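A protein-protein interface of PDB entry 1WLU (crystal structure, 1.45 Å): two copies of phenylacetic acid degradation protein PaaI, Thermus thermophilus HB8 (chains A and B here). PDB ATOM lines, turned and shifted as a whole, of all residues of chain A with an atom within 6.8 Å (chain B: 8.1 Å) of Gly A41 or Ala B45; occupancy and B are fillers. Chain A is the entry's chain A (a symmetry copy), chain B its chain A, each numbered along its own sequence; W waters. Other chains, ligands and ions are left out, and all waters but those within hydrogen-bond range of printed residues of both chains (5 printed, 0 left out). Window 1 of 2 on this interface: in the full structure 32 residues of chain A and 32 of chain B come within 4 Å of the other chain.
Of the 25 printed residues of chain B, 12 touch a printed residue of chain A. Hydrophobic or aromatic side chains of chain A that line the printed part of chain B: Phe A5, Leu A9, His A39, Tyr A44, Ala A45 and Tyr A70. Among the printed residues, 24 pairs touch across the chains.
Gly A40 touches two residues of chain B. Of the printed residues of chain B, Gly A41 touches Phe B5 (3.8 Å), Tyr B44 (3.9 Å), Ala B45 (3.97 Å) and Asp B48 (3.8 Å). Of the printed residues of chain A, His B39 touches Phe A5 and Ala A45. Printed residues of chain A within 4 Å of Gly B40: Tyr A44. Ala B45 touches just these residues of chain A: His A39 (3.9 Å) and Gly A41 (3.97 Å). The nearest printed residue of chain A that does not touch Phe B42 is Ala A45 (5.5 Å).
His A39 touches Ala B45, and with the chains exchanged Ala A45 touches His B39. Gly A40 touches Tyr B44, and with the chains exchanged Tyr A44 touches Gly B40. Tyr A44 touches its own counterpart, Tyr B44. Tyr A44 touches Tyr B70, and with the chains exchanged Tyr A70 touches Tyr B44. Positions printed for both chains: 5, 9, 39, 40, 41, 42, 43, 44, 45, 46 and 70. Of the 24 pairs that touch across the chains among the printed residues, 19 have their exchanged pair printed and touching as well.
Water W3 lies within hydrogen-bond range of the side-chain carboxylate of Asp B48, the side-chain hydroxyl of Tyr B44 and the side-chain hydroxyl of Tyr A70. Water W4 lies within hydrogen-bond range of OD2 of Asp B3, NE2 of His A39, OG of Ser B49 and SD of Met B6. Water W1 lies within hydrogen-bond range of the side-chain hydroxyl (OH) of Tyr A44 (2.8 Å) and the side-chain hydroxyl (OH) of Tyr B70 (3.0 Å). Water W5 lies within hydrogen-bond range of the side-chain carboxylate (OD2) of Asp B48 and a ring nitrogen (NE2) of His A39. Water W2 lies within hydrogen-bond range of the backbone NH (N) of Gly A40 (2.8 Å) and the side-chain carboxylate (OD2) of Asp B48 (3.4 Å).
CD2 of Phe A5 touches CG of His B39, 3.4 Å away. Phe A5 touches Phe B42 (CE2 to N, 3.7 Å). Leu A9 touches Phe B5. His A39 touches Asp B48 (CE1 to OD2, 3.3 Å). Gly A41 touches Phe B5. Tyr B44 touches Gly A41 (CD1 to CA, 3.9 Å). Phe A42 touches Phe B5. CE1 of Tyr A44 touches O of Gly B40, at 3.8 Å. Ala A45 touches His B39. Gly B41 touches Ala A45.
The side-chain hydroxyl (OH) of Tyr B70 lies within hydrogen-bond range of the side-chain hydroxyl (OH) of Tyr A44 (2.9 Å). The side-chain hydroxyl (OG) of Ser B49 lies within hydrogen-bond range of a ring nitrogen (NE2) of His A39 (3.1 Å). The side-chain hydroxyl (OH) of Tyr A70 is in hydrogen-bond range of the side-chain hydroxyl (OH) of Tyr B44 (2.9 Å).
The backbone carbonyl oxygen (O) of Gly B40 lies within hydrogen-bond range of the side-chain hydroxyl (OH) of Tyr B70 (2.9 Å). The backbone carbonyl oxygen (O) of Gly A40 lies within hydrogen-bond range of the side-chain hydroxyl (OH) of Tyr A70, 2.9 Å away. The side-chain hydroxyl of Ser B49 sits at hydrogen-bond distance from the backbone carbonyl oxygen of Ala B45, at 2.8 Å. The side-chain carboxylate (OD1) of Asp B3 lies within hydrogen-bond range of the backbone NH (N) of Phe B5 (3.2 Å). The backbone NH of Gly A41 sits at hydrogen-bond distance from a ring nitrogen (ND1) of His A39, 2.8 Å away. A ring nitrogen (ND1) of His B39 is in hydrogen-bond range of the backbone NH (N) of Gly B41 (2.8 Å).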
ATOM      1  N   PHE A   5      -1.314  11.803 -12.674  1.00  0.00           N
ATOM      2  CA  PHE A   5      -0.617  11.098 -13.744  1.00  0.00           C
ATOM      3  C   PHE A   5      -1.581  10.616 -14.826  1.00  0.00           C
ATOM      4  O   PHE A   5      -1.279  10.700 -16.016  1.00  0.00           O
ATOM      5  CB  PHE A   5       0.188   9.928 -13.170  1.00  0.00           C
ATOM      6  CG  PHE A   5       1.253   9.405 -14.101  1.00  0.00           C
ATOM      7  CD1 PHE A   5       2.158  10.274 -14.711  1.00  0.00           C
ATOM      8  CD2 PHE A   5       1.372   8.041 -14.342  1.00  0.00           C
ATOM      9  CE1 PHE A   5       3.167   9.787 -15.547  1.00  0.00           C
ATOM     10  CE2 PHE A   5       2.377   7.543 -15.175  1.00  0.00           C
ATOM     11  CZ  PHE A   5       3.275   8.419 -15.776  1.00  0.00           C
ATOM     12  N   LEU A   9      -1.431  11.851 -18.727  1.00  0.00           N
ATOM     13  CA  LEU A   9      -1.333  10.901 -19.832  1.00  0.00           C
ATOM     14  C   LEU A   9      -2.557  10.921 -20.744  1.00  0.00           C
ATOM     15  O   LEU A   9      -2.586  10.231 -21.762  1.00  0.00           O
ATOM     16  CB  LEU A   9      -1.128   9.483 -19.292  1.00  0.00           C
ATOM     17  CG  LEU A   9       0.184   9.209 -18.558  1.00  0.00           C
ATOM     18  CD1 LEU A   9       0.203   7.768 -18.066  1.00  0.00           C
ATOM     19  CD2 LEU A   9       1.356   9.469 -19.491  1.00  0.00           C
ATOM     20  N   ALA A  38       4.684   2.588 -28.717  1.00  0.00           N
ATOM     21  CA  ALA A  38       4.220   2.985 -27.394  1.00  0.00           C
ATOM     22  C   ALA A  38       5.181   2.466 -26.328  1.00  0.00           C
ATOM     23  O   ALA A  38       5.471   1.271 -26.267  1.00  0.00           O
ATOM     24  CB  ALA A  38       2.817   2.451 -27.150  1.00  0.00           C
ATOM     25  N   HIS A  39       5.680   3.373 -25.494  1.00  0.00           N
ATOM     26  CA  HIS A  39       6.616   3.018 -24.431  1.00  0.00           C
ATOM     27  C   HIS A  39       5.955   2.018 -23.483  1.00  0.00           C
ATOM     28  O   HIS A  39       4.769   2.141 -23.160  1.00  0.00           O
ATOM     29  CB  HIS A  39       7.026   4.292 -23.681  1.00  0.00           C
ATOM     30  CG  HIS A  39       8.205   4.126 -22.770  1.00  0.00           C
ATOM     31  ND1 HIS A  39       8.148   3.414 -21.591  1.00  0.00           N
ATOM     32  CD2 HIS A  39       9.458   4.637 -22.839  1.00  0.00           C
ATOM     33  CE1 HIS A  39       9.312   3.500 -20.970  1.00  0.00           C
ATOM     34  NE2 HIS A  39      10.124   4.237 -21.708  1.00  0.00           N
ATOM     35  N   GLY A  40       6.721   1.022 -23.051  1.00  0.00           N
ATOM     36  CA  GLY A  40       6.183   0.019 -22.147  1.00  0.00           C
ATOM     37  C   GLY A  40       5.603   0.643 -20.893  1.00  0.00           C
ATOM     38  O   GLY A  40       4.655   0.116 -20.303  1.00  0.00           O
ATOM     39  N   GLY A  41       6.181   1.767 -20.482  1.00  0.00           N
ATOM     40  CA  GLY A  41       5.715   2.461 -19.297  1.00  0.00           C
ATOM     41  C   GLY A  41       4.354   3.098 -19.491  1.00  0.00           C
ATOM     42  O   GLY A  41       3.598   3.260 -18.534  1.00  0.00           O
ATOM     43  N   PHE A  42       4.040   3.478 -20.727  1.00  0.00           N
ATOM     44  CA  PHE A  42       2.741   4.077 -20.996  1.00  0.00           C
ATOM     45  C   PHE A  42       1.678   2.988 -20.932  1.00  0.00           C
ATOM     46  O   PHE A  42       0.630   3.169 -20.311  1.00  0.00           O
ATOM     47  CB  PHE A  42       2.708   4.736 -22.376  1.00  0.00           C
ATOM     48  CG  PHE A  42       1.343   5.223 -22.768  1.00  0.00           C
ATOM     49  CD1 PHE A  42       0.798   6.358 -22.175  1.00  0.00           C
ATOM     50  CD2 PHE A  42       0.575   4.509 -23.681  1.00  0.00           C
ATOM     51  CE1 PHE A  42      -0.497   6.772 -22.484  1.00  0.00           C
ATOM     52  CE2 PHE A  42      -0.721   4.915 -23.996  1.00  0.00           C
ATOM     53  CZ  PHE A  42      -1.257   6.048 -23.395  1.00  0.00           C
ATOM     54  N   LEU A  43       1.945   1.856 -21.578  1.00  0.00           N
ATOM     55  CA  LEU A  43       0.994   0.752 -21.572  1.00  0.00           C
ATOM     56  C   LEU A  43       0.820   0.226 -20.152  1.00  0.00           C
ATOM     57  O   LEU A  43      -0.290  -0.104 -19.735  1.00  0.00           O
ATOM     58  CB  LEU A  43       1.464  -0.361 -22.510  1.00  0.00           C
ATOM     59  CG  LEU A  43       1.548   0.053 -23.984  1.00  0.00           C
ATOM     60  CD1 LEU A  43       2.044  -1.119 -24.811  1.00  0.00           C
ATOM     61  CD2 LEU A  43       0.180   0.519 -24.477  1.00  0.00           C
ATOM     62  N   TYR A  44       1.914   0.154 -19.402  1.00  0.00           N
ATOM     63  CA  TYR A  44       1.827  -0.308 -18.025  1.00  0.00           C
ATOM     64  C   TYR A  44       1.025   0.688 -17.191  1.00  0.00           C
ATOM     65  O   TYR A  44       0.177   0.291 -16.395  1.00  0.00           O
ATOM     66  CB  TYR A  44       3.223  -0.492 -17.422  1.00  0.00           C
ATOM     67  CG  TYR A  44       3.207  -0.960 -15.980  1.00  0.00           C
ATOM     68  CD1 TYR A  44       3.032  -0.055 -14.929  1.00  0.00           C
ATOM     69  CD2 TYR A  44       3.355  -2.309 -15.668  1.00  0.00           C
ATOM     70  CE1 TYR A  44       3.007  -0.486 -13.604  1.00  0.00           C
ATOM     71  CE2 TYR A  44       3.330  -2.751 -14.352  1.00  0.00           C
ATOM     72  CZ  TYR A  44       3.159  -1.838 -13.325  1.00  0.00           C
ATOM     73  OH  TYR A  44       3.152  -2.285 -12.022  1.00  0.00           O
ATOM     74  N   ALA A  45       1.285   1.982 -17.374  1.00  0.00           N
ATOM     75  CA  ALA A  45       0.564   3.002 -16.620  1.00  0.00           C
ATOM     76  C   ALA A  45      -0.937   2.872 -16.855  1.00  0.00           C
ATOM     77  O   ALA A  45      -1.738   3.039 -15.934  1.00  0.00           O
ATOM     78  CB  ALA A  45       1.041   4.391 -17.026  1.00  0.00           C
ATOM     79  N   LEU A  46      -1.311   2.576 -18.094  1.00  0.00           N
ATOM     80  CA  LEU A  46      -2.713   2.404 -18.450  1.00  0.00           C
ATOM     81  C   LEU A  46      -3.305   1.226 -17.678  1.00  0.00           C
ATOM     82  O   LEU A  46      -4.346   1.350 -17.034  1.00  0.00           O
ATOM     83  CB  LEU A  46      -2.840   2.153 -19.954  1.00  0.00           C
ATOM     84  CG  LEU A  46      -4.248   1.914 -20.497  1.00  0.00           C
ATOM     85  CD1 LEU A  46      -5.040   3.215 -20.455  1.00  0.00           C
ATOM     86  CD2 LEU A  46      -4.160   1.402 -21.923  1.00  0.00           C
ATOM     87  N   TYR A  70       3.874  -8.373 -22.735  1.00  0.00           N
ATOM     88  CA  TYR A  70       3.643  -7.628 -23.974  1.00  0.00           C
ATOM     89  C   TYR A  70       3.528  -8.543 -25.184  1.00  0.00           C
ATOM     90  O   TYR A  70       4.401  -9.382 -25.414  1.00  0.00           O
ATOM     91  CB  TYR A  70       4.795  -6.646 -24.189  1.00  0.00           C
ATOM     92  CG  TYR A  70       4.925  -5.604 -23.103  1.00  0.00           C
ATOM     93  CD1 TYR A  70       4.263  -4.383 -23.197  1.00  0.00           C
ATOM     94  CD2 TYR A  70       5.716  -5.838 -21.980  1.00  0.00           C
ATOM     95  CE1 TYR A  70       4.388  -3.416 -22.203  1.00  0.00           C
ATOM     96  CE2 TYR A  70       5.846  -4.881 -20.980  1.00  0.00           C
ATOM     97  CZ  TYR A  70       5.180  -3.672 -21.100  1.00  0.00           C
ATOM     98  OH  TYR A  70       5.310  -2.711 -20.127  1.00  0.00           O
ATOM     99  N   ASP B   3      14.125   9.251 -26.863  1.00  0.00           N
ATOM    100  CA  ASP B   3      12.953   8.574 -26.326  1.00  0.00           C
ATOM    101  C   ASP B   3      11.968   9.641 -25.860  1.00  0.00           C
ATOM    102  O   ASP B   3      12.137  10.237 -24.798  1.00  0.00           O
ATOM    103  CB  ASP B   3      13.356   7.666 -25.162  1.00  0.00           C
ATOM    104  CG  ASP B   3      12.248   6.718 -24.760  1.00  0.00           C
ATOM    105  OD1 ASP B   3      11.179   7.206 -24.338  1.00  0.00           O
ATOM    106  OD2 ASP B   3      12.444   5.487 -24.871  1.00  0.00           O
ATOM    107  N   PHE B   5       8.961   9.561 -24.532  1.00  0.00           N
ATOM    108  CA  PHE B   5       8.346   9.373 -23.223  1.00  0.00           C
ATOM    109  C   PHE B   5       9.327   9.661 -22.089  1.00  0.00           C
ATOM    110  O   PHE B   5       8.962  10.272 -21.085  1.00  0.00           O
ATOM    111  CB  PHE B   5       7.775   7.958 -23.105  1.00  0.00           C
ATOM    112  CG  PHE B   5       6.772   7.794 -21.991  1.00  0.00           C
ATOM    113  CD1 PHE B   5       5.707   8.686 -21.852  1.00  0.00           C
ATOM    114  CD2 PHE B   5       6.873   6.731 -21.100  1.00  0.00           C
ATOM    115  CE1 PHE B   5       4.758   8.515 -20.840  1.00  0.00           C
ATOM    116  CE2 PHE B   5       5.929   6.551 -20.086  1.00  0.00           C
ATOM    117  CZ  PHE B   5       4.871   7.445 -19.958  1.00  0.00           C
ATOM    118  N   MET B   6      10.576   9.225 -22.238  1.00  0.00           N
ATOM    119  CA  MET B   6      11.570   9.509 -21.209  1.00  0.00           C
ATOM    120  C   MET B   6      11.714  11.024 -21.081  1.00  0.00           C
ATOM    121  O   MET B   6      11.782  11.563 -19.979  1.00  0.00           O
ATOM    122  CB  MET B   6      12.926   8.902 -21.578  1.00  0.00           C
ATOM    123  CG  MET B   6      12.998   7.391 -21.432  1.00  0.00           C
ATOM    124  SD  MET B   6      14.638   6.761 -21.823  1.00  0.00           S
ATOM    125  CE  MET B   6      15.567   7.352 -20.434  1.00  0.00           C
ATOM    126  N   LEU B   9       8.796  12.621 -19.311  1.00  0.00           N
ATOM    127  CA  LEU B   9       8.810  12.343 -17.877  1.00  0.00           C
ATOM    128  C   LEU B   9       9.971  13.018 -17.151  1.00  0.00           C
ATOM    129  O   LEU B   9      10.069  12.939 -15.927  1.00  0.00           O
ATOM    130  CB  LEU B   9       8.871  10.832 -17.634  1.00  0.00           C
ATOM    131  CG  LEU B   9       7.657  10.015 -18.075  1.00  0.00           C
ATOM    132  CD1 LEU B   9       7.903   8.540 -17.787  1.00  0.00           C
ATOM    133  CD2 LEU B   9       6.417  10.502 -17.342  1.00  0.00           C
ATOM    134  N   LEU B  11      13.182  12.251 -17.490  1.00  0.00           N
ATOM    135  CA  LEU B  11      14.207  11.281 -17.129  1.00  0.00           C
ATOM    136  C   LEU B  11      15.545  11.571 -17.798  1.00  0.00           C
ATOM    137  O   LEU B  11      15.600  12.144 -18.889  1.00  0.00           O
ATOM    138  CB  LEU B  11      13.740   9.869 -17.495  1.00  0.00           C
ATOM    139  CG  LEU B  11      12.358   9.476 -16.964  1.00  0.00           C
ATOM    140  CD1 LEU B  11      12.090   8.012 -17.298  1.00  0.00           C
ATOM    141  CD2 LEU B  11      12.290   9.702 -15.459  1.00  0.00           C
ATOM    142  N   VAL B  23      19.041   5.095 -15.009  1.00  0.00           N
ATOM    143  CA  VAL B  23      18.171   6.187 -15.429  1.00  0.00           C
ATOM    144  C   VAL B  23      17.655   6.850 -14.164  1.00  0.00           C
ATOM    145  O   VAL B  23      17.301   6.168 -13.202  1.00  0.00           O
ATOM    146  CB  VAL B  23      16.987   5.668 -16.275  1.00  0.00           C
ATOM    147  CG1 VAL B  23      16.005   6.797 -16.562  1.00  0.00           C
ATOM    148  CG2 VAL B  23      17.507   5.084 -17.582  1.00  0.00           C
ATOM    149  N   HIS B  39       2.912   7.557  -8.920  1.00  0.00           N
ATOM    150  CA  HIS B  39       2.098   6.571  -9.624  1.00  0.00           C
ATOM    151  C   HIS B  39       2.960   5.359  -9.981  1.00  0.00           C
ATOM    152  O   HIS B  39       4.121   5.502 -10.375  1.00  0.00           O
ATOM    153  CB  HIS B  39       1.514   7.216 -10.888  1.00  0.00           C
ATOM    154  CG  HIS B  39       0.422   6.425 -11.543  1.00  0.00           C
ATOM    155  ND1 HIS B  39       0.651   5.243 -12.216  1.00  0.00           N
ATOM    156  CD2 HIS B  39      -0.900   6.684 -11.680  1.00  0.00           C
ATOM    157  CE1 HIS B  39      -0.482   4.813 -12.744  1.00  0.00           C
ATOM    158  NE2 HIS B  39      -1.439   5.671 -12.433  1.00  0.00           N
ATOM    159  N   GLY B  40       2.392   4.167  -9.828  1.00  0.00           N
ATOM    160  CA  GLY B  40       3.131   2.955 -10.139  1.00  0.00           C
ATOM    161  C   GLY B  40       3.653   2.963 -11.561  1.00  0.00           C
ATOM    162  O   GLY B  40       4.702   2.380 -11.855  1.00  0.00           O
ATOM    163  N   GLY B  41       2.914   3.620 -12.449  1.00  0.00           N
ATOM    164  CA  GLY B  41       3.310   3.702 -13.842  1.00  0.00           C
ATOM    165  C   GLY B  41       4.534   4.570 -14.050  1.00  0.00           C
ATOM    166  O   GLY B  41       5.295   4.360 -14.995  1.00  0.00           O
ATOM    167  N   PHE B  42       4.724   5.559 -13.181  1.00  0.00           N
ATOM    168  CA  PHE B  42       5.891   6.421 -13.303  1.00  0.00           C
ATOM    169  C   PHE B  42       7.124   5.639 -12.866  1.00  0.00           C
ATOM    170  O   PHE B  42       8.153   5.662 -13.542  1.00  0.00           O
ATOM    171  CB  PHE B  42       5.751   7.672 -12.434  1.00  0.00           C
ATOM    172  CG  PHE B  42       6.996   8.510 -12.397  1.00  0.00           C
ATOM    173  CD1 PHE B  42       7.369   9.275 -13.497  1.00  0.00           C
ATOM    174  CD2 PHE B  42       7.831   8.483 -11.285  1.00  0.00           C
ATOM    175  CE1 PHE B  42       8.561   9.998 -13.493  1.00  0.00           C
ATOM    176  CE2 PHE B  42       9.025   9.203 -11.271  1.00  0.00           C
ATOM    177  CZ  PHE B  42       9.390   9.960 -12.378  1.00  0.00           C
ATOM    178  N   LEU B  43       7.021   4.950 -11.733  1.00  0.00           N
ATOM    179  CA  LEU B  43       8.143   4.166 -11.234  1.00  0.00           C
ATOM    180  C   LEU B  43       8.467   3.043 -12.212  1.00  0.00           C
ATOM    181  O   LEU B  43       9.634   2.741 -12.460  1.00  0.00           O
ATOM    182  CB  LEU B  43       7.825   3.603  -9.847  1.00  0.00           C
ATOM    183  CG  LEU B  43       7.607   4.672  -8.770  1.00  0.00           C
ATOM    184  CD1 LEU B  43       7.278   4.000  -7.450  1.00  0.00           C
ATOM    185  CD2 LEU B  43       8.854   5.544  -8.635  1.00  0.00           C
ATOM    186  N   TYR B  44       7.435   2.427 -12.779  1.00  0.00           N
ATOM    187  CA  TYR B  44       7.660   1.365 -13.748  1.00  0.00           C
ATOM    188  C   TYR B  44       8.320   1.935 -15.001  1.00  0.00           C
ATOM    189  O   TYR B  44       9.258   1.345 -15.532  1.00  0.00           O
ATOM    190  CB  TYR B  44       6.344   0.675 -14.117  1.00  0.00           C
ATOM    191  CG  TYR B  44       6.503  -0.436 -15.137  1.00  0.00           C
ATOM    192  CD1 TYR B  44       6.570  -0.156 -16.504  1.00  0.00           C
ATOM    193  CD2 TYR B  44       6.597  -1.765 -14.732  1.00  0.00           C
ATOM    194  CE1 TYR B  44       6.726  -1.176 -17.442  1.00  0.00           C
ATOM    195  CE2 TYR B  44       6.755  -2.790 -15.656  1.00  0.00           C
ATOM    196  CZ  TYR B  44       6.816  -2.492 -17.006  1.00  0.00           C
ATOM    197  OH  TYR B  44       6.957  -3.517 -17.916  1.00  0.00           O
ATOM    198  N   ALA B  45       7.839   3.084 -15.471  1.00  0.00           N
ATOM    199  CA  ALA B  45       8.412   3.701 -16.664  1.00  0.00           C
ATOM    200  C   ALA B  45       9.902   3.959 -16.463  1.00  0.00           C
ATOM    201  O   ALA B  45      10.704   3.779 -17.381  1.00  0.00           O
ATOM    202  CB  ALA B  45       7.691   5.006 -16.978  1.00  0.00           C
ATOM    203  N   LEU B  46      10.264   4.384 -15.258  1.00  0.00           N
ATOM    204  CA  LEU B  46      11.657   4.648 -14.927  1.00  0.00           C
ATOM    205  C   LEU B  46      12.472   3.361 -15.039  1.00  0.00           C
ATOM    206  O   LEU B  46      13.506   3.323 -15.706  1.00  0.00           O
ATOM    207  CB  LEU B  46      11.757   5.201 -13.504  1.00  0.00           C
ATOM    208  CG  LEU B  46      13.159   5.503 -12.978  1.00  0.00           C
ATOM    209  CD1 LEU B  46      13.723   6.724 -13.694  1.00  0.00           C
ATOM    210  CD2 LEU B  46      13.094   5.758 -11.482  1.00  0.00           C
ATOM    211  N   ALA B  47      11.998   2.302 -14.390  1.00  0.00           N
ATOM    212  CA  ALA B  47      12.697   1.022 -14.423  1.00  0.00           C
ATOM    213  C   ALA B  47      12.745   0.456 -15.835  1.00  0.00           C
ATOM    214  O   ALA B  47      13.782  -0.037 -16.282  1.00  0.00           O
ATOM    215  CB  ALA B  47      12.014   0.034 -13.486  1.00  0.00           C
ATOM    216  N   ASP B  48      11.618   0.531 -16.535  1.00  0.00           N
ATOM    217  CA  ASP B  48      11.520   0.021 -17.894  1.00  0.00           C
ATOM    218  C   ASP B  48      12.483   0.739 -18.831  1.00  0.00           C
ATOM    219  O   ASP B  48      13.027   0.133 -19.754  1.00  0.00           O
ATOM    220  CB  ASP B  48      10.089   0.182 -18.408  1.00  0.00           C
ATOM    221  CG  ASP B  48       9.884  -0.470 -19.752  1.00  0.00           C
ATOM    222  OD1 ASP B  48       9.996  -1.709 -19.826  1.00  0.00           O
ATOM    223  OD2 ASP B  48       9.617   0.250 -20.733  1.00  0.00           O
ATOM    224  N   SER B  49      12.690   2.031 -18.597  1.00  0.00           N
ATOM    225  CA  SER B  49      13.602   2.804 -19.435  1.00  0.00           C
ATOM    226  C   SER B  49      15.044   2.326 -19.254  1.00  0.00           C
ATOM    227  O   SER B  49      15.783   2.201 -20.229  1.00  0.00           O
ATOM    228  CB  SER B  49      13.484   4.296 -19.112  1.00  0.00           C
ATOM    229  OG  SER B  49      12.198   4.785 -19.461  1.00  0.00           O
ATOM    230  N   ALA B  50      15.443   2.061 -18.012  1.00  0.00           N
ATOM    231  CA  ALA B  50      16.794   1.571 -17.746  1.00  0.00           C
ATOM    232  C   ALA B  50      16.934   0.174 -18.360  1.00  0.00           C
ATOM    233  O   ALA B  50      17.968  -0.168 -18.931  1.00  0.00           O
ATOM    234  CB  ALA B  50      17.045   1.521 -16.246  1.00  0.00           C
ATOM    235  N   PHE B  51      15.874  -0.620 -18.230  1.00  0.00           N
ATOM    236  CA  PHE B  51      15.788  -1.976 -18.770  1.00  0.00           C
ATOM    237  C   PHE B  51      15.954  -1.937 -20.293  1.00  0.00           C
ATOM    238  O   PHE B  51      16.719  -2.714 -20.870  1.00  0.00           O
ATOM    239  CB  PHE B  51      14.416  -2.542 -18.364  1.00  0.00           C
ATOM    240  CG  PHE B  51      13.995  -3.792 -19.091  1.00  0.00           C
ATOM    241  CD1 PHE B  51      14.714  -4.975 -18.969  1.00  0.00           C
ATOM    242  CD2 PHE B  51      12.808  -3.803 -19.815  1.00  0.00           C
ATOM    243  CE1 PHE B  51      14.248  -6.152 -19.548  1.00  0.00           C
ATOM    244  CE2 PHE B  51      12.334  -4.976 -20.399  1.00  0.00           C
ATOM    245  CZ  PHE B  51      13.056  -6.151 -20.262  1.00  0.00           C
ATOM    246  N   ALA B  52      15.243  -1.013 -20.933  1.00  0.00           N
ATOM    247  CA  ALA B  52      15.306  -0.856 -22.380  1.00  0.00           C
ATOM    248  C   ALA B  52      16.708  -0.486 -22.850  1.00  0.00           C
ATOM    249  O   ALA B  52      17.239  -1.087 -23.784  1.00  0.00           O
ATOM    250  CB  ALA B  52      14.317   0.212 -22.825  1.00  0.00           C
ATOM    251  N   MET B  68       7.198  -6.072 -11.490  1.00  0.00           N
ATOM    252  CA  MET B  68       7.522  -4.908 -10.686  1.00  0.00           C
ATOM    253  C   MET B  68       7.023  -5.152  -9.265  1.00  0.00           C
ATOM    254  O   MET B  68       5.823  -5.347  -9.049  1.00  0.00           O
ATOM    255  CB  MET B  68       6.847  -3.664 -11.270  1.00  0.00           C
ATOM    256  CG  MET B  68       7.186  -2.373 -10.554  1.00  0.00           C
ATOM    257  SD  MET B  68       8.871  -1.825 -10.867  1.00  0.00           S
ATOM    258  CE  MET B  68       8.749  -0.113 -10.324  1.00  0.00           C
ATOM    259  N   TYR B  70       6.787  -3.518  -5.574  1.00  0.00           N
ATOM    260  CA  TYR B  70       6.833  -2.230  -4.879  1.00  0.00           C
ATOM    261  C   TYR B  70       7.046  -2.391  -3.381  1.00  0.00           C
ATOM    262  O   TYR B  70       6.316  -3.138  -2.726  1.00  0.00           O
ATOM    263  CB  TYR B  70       5.525  -1.480  -5.127  1.00  0.00           C
ATOM    264  CG  TYR B  70       5.271  -1.152  -6.580  1.00  0.00           C
ATOM    265  CD1 TYR B  70       5.713   0.046  -7.133  1.00  0.00           C
ATOM    266  CD2 TYR B  70       4.581  -2.040  -7.402  1.00  0.00           C
ATOM    267  CE1 TYR B  70       5.472   0.356  -8.469  1.00  0.00           C
ATOM    268  CE2 TYR B  70       4.337  -1.742  -8.738  1.00  0.00           C
ATOM    269  CZ  TYR B  70       4.785  -0.541  -9.263  1.00  0.00           C
ATOM    270  OH  TYR B  70       4.539  -0.226 -10.577  1.00  0.00           O
ATOM    271  N   ALA B  82      16.932   4.137 -11.368  1.00  0.00           N
ATOM    272  CA  ALA B  82      16.667   2.752 -11.740  1.00  0.00           C
ATOM    273  C   ALA B  82      17.994   2.222 -12.277  1.00  0.00           C
ATOM    274  O   ALA B  82      18.519   2.723 -13.276  1.00  0.00           O
ATOM    275  CB  ALA B  82      15.589   2.675 -12.805  1.00  0.00           C
ATOM    276  N   VAL B 100      15.198  -0.034  -8.124  1.00  0.00           N
ATOM    277  CA  VAL B 100      14.709   1.342  -8.081  1.00  0.00           C
ATOM    278  C   VAL B 100      15.071   1.849  -6.692  1.00  0.00           C
ATOM    279  O   VAL B 100      14.580   1.337  -5.680  1.00  0.00           O
ATOM    280  CB  VAL B 100      13.187   1.398  -8.319  1.00  0.00           C
ATOM    281  CG1 VAL B 100      12.706   2.839  -8.307  1.00  0.00           C
ATOM    282  CG2 VAL B 100      12.860   0.752  -9.662  1.00  0.00           C
ATOM    283  N   PHE B 110      12.500  -4.494 -10.185  1.00  0.00           N
ATOM    284  CA  PHE B 110      11.959  -4.816 -11.499  1.00  0.00           C
ATOM    285  C   PHE B 110      12.780  -5.962 -12.084  1.00  0.00           C
ATOM    286  O   PHE B 110      14.005  -5.974 -11.992  1.00  0.00           O
ATOM    287  CB  PHE B 110      12.035  -3.542 -12.364  1.00  0.00           C
ATOM    288  CG  PHE B 110      11.695  -3.734 -13.821  1.00  0.00           C
ATOM    289  CD1 PHE B 110      12.561  -4.416 -14.675  1.00  0.00           C
ATOM    290  CD2 PHE B 110      10.556  -3.139 -14.361  1.00  0.00           C
ATOM    291  CE1 PHE B 110      12.299  -4.494 -16.044  1.00  0.00           C
ATOM    292  CE2 PHE B 110      10.289  -3.212 -15.728  1.00  0.00           C
ATOM    293  CZ  PHE B 110      11.164  -3.889 -16.568  1.00  0.00           C
HETATM  294  O   HOH W   1       1.765  -1.109  -9.937  1.00  0.00           O
HETATM  295  O   HOH W   2       9.306   0.839 -24.097  1.00  0.00           O
HETATM  296  O   HOH W   3       8.219  -3.315 -20.369  1.00  0.00           O
HETATM  297  O   HOH W   4      12.859   3.913 -22.727  1.00  0.00           O
HETATM  298  O   HOH W   5      11.273   1.523 -22.560  1.00  0.00           O
